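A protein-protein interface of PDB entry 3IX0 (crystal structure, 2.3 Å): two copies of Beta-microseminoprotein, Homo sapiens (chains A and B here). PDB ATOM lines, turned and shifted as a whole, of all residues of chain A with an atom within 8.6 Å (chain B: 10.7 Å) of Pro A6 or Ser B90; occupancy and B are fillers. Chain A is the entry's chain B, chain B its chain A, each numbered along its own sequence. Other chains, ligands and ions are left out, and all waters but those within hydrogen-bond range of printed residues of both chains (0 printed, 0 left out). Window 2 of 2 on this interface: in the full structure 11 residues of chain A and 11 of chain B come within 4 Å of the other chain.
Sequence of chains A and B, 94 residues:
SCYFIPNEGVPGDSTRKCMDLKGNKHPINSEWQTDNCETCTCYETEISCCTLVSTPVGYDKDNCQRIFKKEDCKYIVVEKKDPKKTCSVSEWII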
ATOM      1  N   TYR A   3      16.123 -18.767  -7.523  1.00  0.00           N
ATOM      2  CA  TYR A   3      16.384 -17.675  -6.602  1.00  0.00           C
ATOM      3  C   TYR A   3      16.735 -16.439  -7.402  1.00  0.00           C
ATOM      4  O   TYR A   3      17.167 -16.550  -8.539  1.00  0.00           O
ATOM      5  CB  TYR A   3      17.461 -18.011  -5.544  1.00  0.00           C
ATOM      6  CG  TYR A   3      18.885 -18.237  -6.038  1.00  0.00           C
ATOM      7  CD1 TYR A   3      19.687 -17.170  -6.407  1.00  0.00           C
ATOM      8  CD2 TYR A   3      19.446 -19.521  -6.082  1.00  0.00           C
ATOM      9  CE1 TYR A   3      21.002 -17.358  -6.829  1.00  0.00           C
ATOM     10  CE2 TYR A   3      20.762 -19.723  -6.512  1.00  0.00           C
ATOM     11  CZ  TYR A   3      21.528 -18.634  -6.884  1.00  0.00           C
ATOM     12  OH  TYR A   3      22.819 -18.795  -7.311  1.00  0.00           O
ATOM     13  N   PHE A   4      16.499 -15.272  -6.799  1.00  0.00           N
ATOM     14  CA  PHE A   4      16.854 -13.978  -7.361  1.00  0.00           C
ATOM     15  C   PHE A   4      17.593 -13.180  -6.288  1.00  0.00           C
ATOM     16  O   PHE A   4      17.095 -13.010  -5.174  1.00  0.00           O
ATOM     17  CB  PHE A   4      15.610 -13.202  -7.791  1.00  0.00           C
ATOM     18  CG  PHE A   4      14.847 -13.835  -8.922  1.00  0.00           C
ATOM     19  CD1 PHE A   4      14.872 -13.277 -10.195  1.00  0.00           C
ATOM     20  CD2 PHE A   4      14.096 -14.977  -8.713  1.00  0.00           C
ATOM     21  CE1 PHE A   4      14.166 -13.862 -11.242  1.00  0.00           C
ATOM     22  CE2 PHE A   4      13.382 -15.558  -9.748  1.00  0.00           C
ATOM     23  CZ  PHE A   4      13.422 -15.001 -11.012  1.00  0.00           C
ATOM     24  N   ILE A   5      18.787 -12.706  -6.622  1.00  0.00           N
ATOM     25  CA  ILE A   5      19.584 -11.914  -5.704  1.00  0.00           C
ATOM     26  C   ILE A   5      20.041 -10.673  -6.442  1.00  0.00           C
ATOM     27  O   ILE A   5      20.006 -10.622  -7.681  1.00  0.00           O
ATOM     28  CB  ILE A   5      20.832 -12.674  -5.219  1.00  0.00           C
ATOM     29  CG1 ILE A   5      21.586 -13.228  -6.427  1.00  0.00           C
ATOM     30  CG2 ILE A   5      20.440 -13.780  -4.261  1.00  0.00           C
ATOM     31  CD1 ILE A   5      22.950 -13.831  -6.112  1.00  0.00           C
ATOM     32  N   PRO A   6      20.469  -9.665  -5.682  1.00  0.00           N
ATOM     33  CA  PRO A   6      20.934  -8.405  -6.260  1.00  0.00           C
ATOM     34  C   PRO A   6      22.132  -8.655  -7.146  1.00  0.00           C
ATOM     35  O   PRO A   6      22.911  -9.548  -6.856  1.00  0.00           O
ATOM     36  CB  PRO A   6      21.395  -7.606  -5.033  1.00  0.00           C
ATOM     37  CG  PRO A   6      20.668  -8.222  -3.864  1.00  0.00           C
ATOM     38  CD  PRO A   6      20.539  -9.676  -4.210  1.00  0.00           C
ATOM     39  N   ASN A   7      22.265  -7.886  -8.219  1.00  0.00           N
ATOM     40  CA  ASN A   7      23.500  -7.849  -8.979  1.00  0.00           C
ATOM     41  C   ASN A   7      24.412  -6.727  -8.448  1.00  0.00           C
ATOM     42  O   ASN A   7      24.147  -5.549  -8.650  1.00  0.00           O
ATOM     43  CB  ASN A   7      23.205  -7.631 -10.459  1.00  0.00           C
ATOM     44  CG  ASN A   7      24.467  -7.553 -11.285  1.00  0.00           C
ATOM     45  OD1 ASN A   7      25.525  -7.962 -10.825  1.00  0.00           O
ATOM     46  ND2 ASN A   7      24.368  -7.026 -12.508  1.00  0.00           N
ATOM     47  N   GLU A   8      25.481  -7.077  -7.755  1.00  0.00           N
ATOM     48  CA  GLU A   8      26.388  -6.036  -7.276  1.00  0.00           C
ATOM     49  C   GLU A   8      27.456  -5.693  -8.302  1.00  0.00           C
ATOM     50  O   GLU A   8      28.185  -4.720  -8.139  1.00  0.00           O
ATOM     51  CB  GLU A   8      27.031  -6.420  -5.949  1.00  0.00           C
ATOM     52  CG  GLU A   8      26.087  -6.285  -4.780  1.00  0.00           C
ATOM     53  CD  GLU A   8      26.818  -6.261  -3.464  1.00  0.00           C
ATOM     54  OE1 GLU A   8      27.981  -6.731  -3.428  1.00  0.00           O
ATOM     55  OE2 GLU A   8      26.230  -5.770  -2.474  1.00  0.00           O
ATOM     56  N   GLY A   9      27.526  -6.488  -9.367  1.00  0.00           N
ATOM     57  CA  GLY A   9      28.563  -6.337 -10.368  1.00  0.00           C
ATOM     58  C   GLY A   9      29.896  -6.621  -9.707  1.00  0.00           C
ATOM     59  O   GLY A   9      29.943  -7.256  -8.644  1.00  0.00           O
ATOM     60  N   CYS A  18      27.682  -9.411 -14.446  1.00  0.00           N
ATOM     61  CA  CYS A  18      27.484 -10.260 -13.277  1.00  0.00           C
ATOM     62  C   CYS A  18      28.656 -11.211 -13.123  1.00  0.00           C
ATOM     63  O   CYS A  18      29.080 -11.837 -14.097  1.00  0.00           O
ATOM     64  CB  CYS A  18      26.189 -11.082 -13.402  1.00  0.00           C
ATOM     65  SG  CYS A  18      24.697 -10.118 -13.765  1.00  0.00           S
ATOM     66  N   MET A  19      29.173 -11.329 -11.904  1.00  0.00           N
ATOM     67  CA  MET A  19      30.162 -12.358 -11.612  1.00  0.00           C
ATOM     68  C   MET A  19      29.508 -13.592 -11.009  1.00  0.00           C
ATOM     69  O   MET A  19      28.676 -13.484 -10.109  1.00  0.00           O
ATOM     70  CB  MET A  19      31.246 -11.843 -10.667  1.00  0.00           C
ATOM     71  CG  MET A  19      32.232 -12.943 -10.266  1.00  0.00           C
ATOM     72  SD  MET A  19      33.871 -12.387  -9.761  1.00  0.00           S
ATOM     73  CE  MET A  19      34.595 -11.960 -11.346  1.00  0.00           C
ATOM     74  N   TYR A  43      21.059  -9.943 -15.022  1.00  0.00           N
ATOM     75  CA  TYR A  43      20.389  -8.697 -15.383  1.00  0.00           C
ATOM     76  C   TYR A  43      21.058  -7.521 -14.717  1.00  0.00           C
ATOM     77  O   TYR A  43      21.802  -7.656 -13.724  1.00  0.00           O
ATOM     78  CB  TYR A  43      18.912  -8.671 -14.948  1.00  0.00           C
ATOM     79  CG  TYR A  43      18.084  -9.838 -15.415  1.00  0.00           C
ATOM     80  CD1 TYR A  43      17.924 -10.957 -14.612  1.00  0.00           C
ATOM     81  CD2 TYR A  43      17.463  -9.824 -16.654  1.00  0.00           C
ATOM     82  CE1 TYR A  43      17.174 -12.036 -15.033  1.00  0.00           C
ATOM     83  CE2 TYR A  43      16.707 -10.902 -17.083  1.00  0.00           C
ATOM     84  CZ  TYR A  43      16.563 -12.002 -16.268  1.00  0.00           C
ATOM     85  OH  TYR A  43      15.815 -13.085 -16.689  1.00  0.00           O
ATOM     86  N   GLU A  44      20.738  -6.360 -15.265  1.00  0.00           N
ATOM     87  CA  GLU A  44      21.153  -5.086 -14.723  1.00  0.00           C
ATOM     88  C   GLU A  44      21.107  -5.107 -13.193  1.00  0.00           C
ATOM     89  O   GLU A  44      22.119  -4.898 -12.537  1.00  0.00           O
ATOM     90  CB  GLU A  44      20.236  -3.999 -15.284  1.00  0.00           C
ATOM     91  CG  GLU A  44      20.820  -2.613 -15.288  1.00  0.00           C
ATOM     92  CD  GLU A  44      22.060  -2.507 -16.147  1.00  0.00           C
ATOM     93  OE1 GLU A  44      23.125  -2.122 -15.608  1.00  0.00           O
ATOM     94  OE2 GLU A  44      21.965  -2.810 -17.356  1.00  0.00           O
ATOM     95  N   THR A  45      19.947  -5.407 -12.618  1.00  0.00           N
ATOM     96  CA  THR A  45      19.795  -5.261 -11.180  1.00  0.00           C
ATOM     97  C   THR A  45      19.703  -6.560 -10.393  1.00  0.00           C
ATOM     98  O   THR A  45      19.614  -6.531  -9.171  1.00  0.00           O
ATOM     99  CB  THR A  45      18.558  -4.418 -10.850  1.00  0.00           C
ATOM    100  OG1 THR A  45      17.403  -5.059 -11.398  1.00  0.00           O
ATOM    101  CG2 THR A  45      18.707  -3.026 -11.451  1.00  0.00           C
ATOM    102  N   GLU A  46      19.741  -7.696 -11.078  1.00  0.00           N
ATOM    103  CA  GLU A  46      19.571  -8.961 -10.388  1.00  0.00           C
ATOM    104  C   GLU A  46      20.203 -10.135 -11.119  1.00  0.00           C
ATOM    105  O   GLU A  46      20.466 -10.066 -12.314  1.00  0.00           O
ATOM    106  CB  GLU A  46      18.077  -9.248 -10.168  1.00  0.00           C
ATOM    107  CG  GLU A  46      17.249  -9.321 -11.438  1.00  0.00           C
ATOM    108  CD  GLU A  46      15.788  -9.691 -11.167  1.00  0.00           C
ATOM    109  OE1 GLU A  46      15.349  -9.619 -10.000  1.00  0.00           O
ATOM    110  OE2 GLU A  46      15.077 -10.061 -12.124  1.00  0.00           O
ATOM    111  N   ILE A  47      20.424 -11.214 -10.380  1.00  0.00           N
ATOM    112  CA  ILE A  47      20.835 -12.471 -10.946  1.00  0.00           C
ATOM    113  C   ILE A  47      19.831 -13.509 -10.481  1.00  0.00           C
ATOM    114  O   ILE A  47      19.486 -13.565  -9.300  1.00  0.00           O
ATOM    115  CB  ILE A  47      22.234 -12.882 -10.454  1.00  0.00           C
ATOM    116  CG1 ILE A  47      23.266 -11.791 -10.765  1.00  0.00           C
ATOM    117  CG2 ILE A  47      22.666 -14.194 -11.112  1.00  0.00           C
ATOM    118  CD1 ILE A  47      24.567 -11.981 -10.016  1.00  0.00           C
ATOM    119  N   SER A  48      19.350 -14.322 -11.414  1.00  0.00           N
ATOM    120  CA  SER A  48      18.499 -15.438 -11.065  1.00  0.00           C
ATOM    121  C   SER A  48      19.175 -16.750 -11.472  1.00  0.00           C
ATOM    122  O   SER A  48      19.848 -16.826 -12.491  1.00  0.00           O
ATOM    123  CB  SER A  48      17.151 -15.313 -11.768  1.00  0.00           C
ATOM    124  OG  SER A  48      17.310 -15.470 -13.166  1.00  0.00           O
ATOM    125  N   THR B  55       8.490 -15.482  -3.415  1.00  0.00           N
ATOM    126  CA  THR B  55       8.560 -15.347  -1.979  1.00  0.00           C
ATOM    127  C   THR B  55       9.851 -14.672  -1.582  1.00  0.00           C
ATOM    128  O   THR B  55      10.929 -15.139  -1.918  1.00  0.00           O
ATOM    129  CB  THR B  55       8.466 -16.708  -1.291  1.00  0.00           C
ATOM    130  OG1 THR B  55       7.233 -17.340  -1.677  1.00  0.00           O
ATOM    131  CG2 THR B  55       8.528 -16.532   0.219  1.00  0.00           C
ATOM    132  N   PRO B  56       9.742 -13.547  -0.868  1.00  0.00           N
ATOM    133  CA  PRO B  56      10.933 -12.859  -0.364  1.00  0.00           C
ATOM    134  C   PRO B  56      11.427 -13.598   0.854  1.00  0.00           C
ATOM    135  O   PRO B  56      10.624 -13.946   1.712  1.00  0.00           O
ATOM    136  CB  PRO B  56      10.391 -11.486   0.057  1.00  0.00           C
ATOM    137  CG  PRO B  56       8.978 -11.745   0.433  1.00  0.00           C
ATOM    138  CD  PRO B  56       8.491 -12.897  -0.434  1.00  0.00           C
ATOM    139  N   VAL B  57      12.720 -13.855   0.936  1.00  0.00           N
ATOM    140  CA  VAL B  57      13.247 -14.606   2.069  1.00  0.00           C
ATOM    141  C   VAL B  57      14.428 -13.890   2.708  1.00  0.00           C
ATOM    142  O   VAL B  57      14.790 -14.177   3.839  1.00  0.00           O
ATOM    143  CB  VAL B  57      13.673 -16.022   1.661  1.00  0.00           C
ATOM    144  CG1 VAL B  57      12.463 -16.840   1.295  1.00  0.00           C
ATOM    145  CG2 VAL B  57      14.649 -15.962   0.499  1.00  0.00           C
ATOM    146  N   GLY B  58      15.032 -12.969   1.970  1.00  0.00           N
ATOM    147  CA  GLY B  58      16.176 -12.236   2.463  1.00  0.00           C
ATOM    148  C   GLY B  58      15.818 -10.809   2.807  1.00  0.00           C
ATOM    149  O   GLY B  58      15.774  -9.944   1.933  1.00  0.00           O
ATOM    150  N   TYR B  59      15.566 -10.562   4.090  1.00  0.00           N
ATOM    151  CA  TYR B  59      15.205  -9.226   4.555  1.00  0.00           C
ATOM    152  C   TYR B  59      15.285  -9.116   6.095  1.00  0.00           C
ATOM    153  O   TYR B  59      15.451 -10.125   6.790  1.00  0.00           O
ATOM    154  CB  TYR B  59      13.819  -8.847   4.030  1.00  0.00           C
ATOM    155  CG  TYR B  59      12.711  -9.774   4.495  1.00  0.00           C
ATOM    156  CD1 TYR B  59      12.012  -9.517   5.668  1.00  0.00           C
ATOM    157  CD2 TYR B  59      12.359 -10.901   3.760  1.00  0.00           C
ATOM    158  CE1 TYR B  59      10.999 -10.350   6.099  1.00  0.00           C
ATOM    159  CE2 TYR B  59      11.356 -11.742   4.182  1.00  0.00           C
ATOM    160  CZ  TYR B  59      10.676 -11.462   5.354  1.00  0.00           C
ATOM    161  OH  TYR B  59       9.677 -12.301   5.784  1.00  0.00           O
ATOM    162  N   ASP B  60      15.196  -7.895   6.625  1.00  0.00           N
ATOM    163  CA  ASP B  60      15.249  -7.672   8.079  1.00  0.00           C
ATOM    164  C   ASP B  60      13.957  -8.162   8.734  1.00  0.00           C
ATOM    165  O   ASP B  60      12.938  -7.471   8.693  1.00  0.00           O
ATOM    166  CB  ASP B  60      15.445  -6.187   8.371  1.00  0.00           C
ATOM    167  CG  ASP B  60      15.612  -5.881   9.862  1.00  0.00           C
ATOM    168  OD1 ASP B  60      15.497  -6.782  10.711  1.00  0.00           O
ATOM    169  OD2 ASP B  60      15.871  -4.707  10.177  1.00  0.00           O
ATOM    170  N   LYS B  61      14.010  -9.340   9.349  1.00  0.00           N
ATOM    171  CA  LYS B  61      12.817  -9.986   9.888  1.00  0.00           C
ATOM    172  C   LYS B  61      12.434  -9.530  11.297  1.00  0.00           C
ATOM    173  O   LYS B  61      11.365  -9.882  11.785  1.00  0.00           O
ATOM    174  CB  LYS B  61      12.965 -11.512   9.860  1.00  0.00           C
ATOM    175  CG  LYS B  61      13.062 -12.099   8.456  1.00  0.00           C
ATOM    176  CD  LYS B  61      12.940 -13.624   8.451  1.00  0.00           C
ATOM    177  CE  LYS B  61      13.120 -14.176   7.043  1.00  0.00           C
ATOM    178  NZ  LYS B  61      13.028 -15.663   6.998  1.00  0.00           N
ATOM    179  N   CYS B  64      10.918  -5.966   9.902  1.00  0.00           N
ATOM    180  CA  CYS B  64      10.119  -6.022   8.689  1.00  0.00           C
ATOM    181  C   CYS B  64       9.284  -7.300   8.595  1.00  0.00           C
ATOM    182  O   CYS B  64       9.588  -8.326   9.215  1.00  0.00           O
ATOM    183  CB  CYS B  64      11.013  -5.867   7.454  1.00  0.00           C
ATOM    184  SG  CYS B  64      11.990  -4.347   7.436  1.00  0.00           S
ATOM    185  N   VAL B  77       7.140  -6.396   1.401  1.00  0.00           N
ATOM    186  CA  VAL B  77       7.874  -6.541   2.636  1.00  0.00           C
ATOM    187  C   VAL B  77       7.973  -5.147   3.234  1.00  0.00           C
ATOM    188  O   VAL B  77       8.529  -4.232   2.619  1.00  0.00           O
ATOM    189  CB  VAL B  77       9.286  -7.083   2.404  1.00  0.00           C
ATOM    190  CG1 VAL B  77      10.060  -7.075   3.701  1.00  0.00           C
ATOM    191  CG2 VAL B  77       9.230  -8.489   1.803  1.00  0.00           C
ATOM    192  N   THR B  86       8.391   0.493   2.948  1.00  0.00           N
ATOM    193  CA  THR B  86       8.951  -0.760   2.450  1.00  0.00           C
ATOM    194  C   THR B  86      10.346  -1.009   3.002  1.00  0.00           C
ATOM    195  O   THR B  86      11.077  -0.074   3.307  1.00  0.00           O
ATOM    196  CB  THR B  86       8.998  -0.801   0.901  1.00  0.00           C
ATOM    197  OG1 THR B  86      10.031   0.064   0.429  1.00  0.00           O
ATOM    198  CG2 THR B  86       7.683  -0.351   0.314  1.00  0.00           C
ATOM    199  N   CYS B  87      10.694  -2.280   3.153  1.00  0.00           N
ATOM    200  CA  CYS B  87      12.044  -2.690   3.511  1.00  0.00           C
ATOM    201  C   CYS B  87      12.696  -3.308   2.288  1.00  0.00           C
ATOM    202  O   CYS B  87      12.010  -3.861   1.427  1.00  0.00           O
ATOM    203  CB  CYS B  87      12.011  -3.707   4.637  1.00  0.00           C
ATOM    204  SG  CYS B  87      11.106  -3.094   6.111  1.00  0.00           S
ATOM    205  N   SER B  88      14.019  -3.206   2.205  1.00  0.00           N
ATOM    206  CA  SER B  88      14.741  -3.741   1.062  1.00  0.00           C
ATOM    207  C   SER B  88      14.911  -5.240   1.222  1.00  0.00           C
ATOM    208  O   SER B  88      15.095  -5.736   2.332  1.00  0.00           O
ATOM    209  CB  SER B  88      16.111  -3.082   0.935  1.00  0.00           C
ATOM    210  OG  SER B  88      17.025  -3.667   1.848  1.00  0.00           O
ATOM    211  N   VAL B  89      14.851  -5.952   0.105  1.00  0.00           N
ATOM    212  CA  VAL B  89      14.955  -7.407   0.100  1.00  0.00           C
ATOM    213  C   VAL B  89      16.193  -7.834  -0.684  1.00  0.00           C
ATOM    214  O   VAL B  89      16.474  -7.308  -1.748  1.00  0.00           O
ATOM    215  CB  VAL B  89      13.668  -8.048  -0.501  1.00  0.00           C
ATOM    216  CG1 VAL B  89      13.792  -9.556  -0.578  1.00  0.00           C
ATOM    217  CG2 VAL B  89      12.435  -7.667   0.329  1.00  0.00           C
ATOM    218  N   SER B  90      16.936  -8.784  -0.143  1.00  0.00           N
ATOM    219  CA  SER B  90      18.175  -9.214  -0.755  1.00  0.00           C
ATOM    220  C   SER B  90      18.044 -10.576  -1.448  1.00  0.00           C
ATOM    221  O   SER B  90      18.984 -11.044  -2.082  1.00  0.00           O
ATOM    222  CB  SER B  90      19.255  -9.313   0.313  1.00  0.00           C
ATOM    223  OG  SER B  90      18.833 -10.196   1.341  1.00  0.00           O
ATOM    224  N   GLU B  91      16.891 -11.222  -1.311  1.00  0.00           N
ATOM    225  CA  GLU B  91      16.675 -12.493  -1.993  1.00  0.00           C
ATOM    226  C   GLU B  91      15.199 -12.894  -2.124  1.00  0.00           C
ATOM    227  O   GLU B  91      14.421 -12.825  -1.171  1.00  0.00           O
ATOM    228  CB  GLU B  91      17.448 -13.603  -1.305  1.00  0.00           C
ATOM    229  CG  GLU B  91      17.361 -14.947  -2.031  1.00  0.00           C
ATOM    230  CD  GLU B  91      18.074 -16.057  -1.282  1.00  0.00           C
ATOM    231  OE1 GLU B  91      18.951 -15.756  -0.462  1.00  0.00           O
ATOM    232  OE2 GLU B  91      17.765 -17.237  -1.511  1.00  0.00           O
ATOM    233  N   TRP B  92      14.829 -13.311  -3.321  1.00  0.00           N
ATOM    234  CA  TRP B  92      13.507 -13.855  -3.564  1.00  0.00           C
ATOM    235  C   TRP B  92      13.653 -15.283  -4.050  1.00  0.00           C
ATOM    236  O   TRP B  92      14.666 -15.655  -4.634  1.00  0.00           O
ATOM    237  CB  TRP B  92      12.762 -13.040  -4.626  1.00  0.00           C
ATOM    238  CG  TRP B  92      12.616 -11.589  -4.281  1.00  0.00           C
ATOM    239  CD1 TRP B  92      13.577 -10.621  -4.363  1.00  0.00           C
ATOM    240  CD2 TRP B  92      11.434 -10.941  -3.806  1.00  0.00           C
ATOM    241  NE1 TRP B  92      13.056  -9.411  -3.985  1.00  0.00           N
ATOM    242  CE2 TRP B  92      11.744  -9.581  -3.632  1.00  0.00           C
ATOM    243  CE3 TRP B  92      10.142 -11.381  -3.512  1.00  0.00           C
ATOM    244  CZ2 TRP B  92      10.805  -8.650  -3.178  1.00  0.00           C
ATOM    245  CZ3 TRP B  92       9.206 -10.447  -3.064  1.00  0.00           C
ATOM    246  CH2 TRP B  92       9.545  -9.105  -2.899  1.00  0.00           C
ATOM    247  N   ILE B  93      12.622 -16.076  -3.810  1.00  0.00           N
ATOM    248  CA  ILE B  93      12.584 -17.436  -4.289  1.00  0.00           C
ATOM    249  C   ILE B  93      11.245 -17.687  -4.945  1.00  0.00           C
ATOM    250  O   ILE B  93      10.201 -17.230  -4.442  1.00  0.00           O
ATOM    251  CB  ILE B  93      12.759 -18.429  -3.151  1.00  0.00           C
ATOM    252  CG1 ILE B  93      14.218 -18.473  -2.722  1.00  0.00           C
ATOM    253  CG2 ILE B  93      12.359 -19.815  -3.602  1.00  0.00           C
ATOM    254  CD1 ILE B  93      14.543 -19.664  -1.856  1.00  0.00           C
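O of Trp B92 lies within hydrogen-bond range of N of Phe A4.
N of Val B57 lies within hydrogen-bond range of O of Glu B91 (2.9 Å).
The backbone carbonyl oxygen (O) of Gly B58 sits at hydrogen-bond distance from the backbone NH (N) of Ser B90 (2.6 Å).
The backbone NH (N) of Gly B58 sits at hydrogen-bond distance from the backbone carbonyl oxygen (O) of Glu B91.
N of Ile A47 is in hydrogen-bond range of O of Ile A5 (2.8 Å).
SG of Cys B87 is disulfide-bonded to SG of Cys B64 (2.0 Å).
Among the printed residues, merely in contact across the chains: Tyr A3 with Trp B92 (3.3 Å), Phe A4 with Glu B91 (3.2 Å), Ile A5 with Ser B90 (3.8 Å), Ile A5 with Glu B91 (3.98 Å) and Pro A6 with Ser B90 (3.0 Å).
Of the printed residues of chain B, Phe A4 touches Glu B91 (3.2 Å) and Trp B92 (2.9 Å).
Ile A5 touches two residues of chain B.
Pro A6 touches one residue of chain B.
Cys A18 touches none of the printed residues of chain B.
No residue of chain B comes within 4 Å of Ile A47.
Cys B87 touches none of the printed residues of chain A.
Ser B90 touches just these residues of chain A: Ile A5 and Pro A6.
Of the printed residues of chain A, Trp B92 touches Tyr A3 and Phe A4.
The nearest residue of chain B that does not touch Pro A6 is Val B89 (4.8 Å).
The nearest residue of chain A that does not touch Ser B90 is Phe A4 (4.1 Å).
The nearest printed residue of chain B that does not touch Phe A4 is Ser B90 (4.1 Å).
Printed residues of chain A that touch a printed residue of chain B: Tyr A3, Phe A4, Ile A5 and Pro A6.
Hydrophobic or aromatic side chains of chain A within 4 Å of the printed part of chain B: Tyr A3, Ile A5 and Pro A6.
Of the 17 printed residues of chain B, 3 touch a printed residue of chain A.
Along chain B the printed residues that touch a printed residue of chain A span positions 90 to 92.
Among the printed residues, 6 pairs touch across the chains.
Among the printed residues, no Asp or Glu carboxylate lies within 4 Å of a Lys or Arg side-chain nitrogen of the other chain.
No position is printed for both chains.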
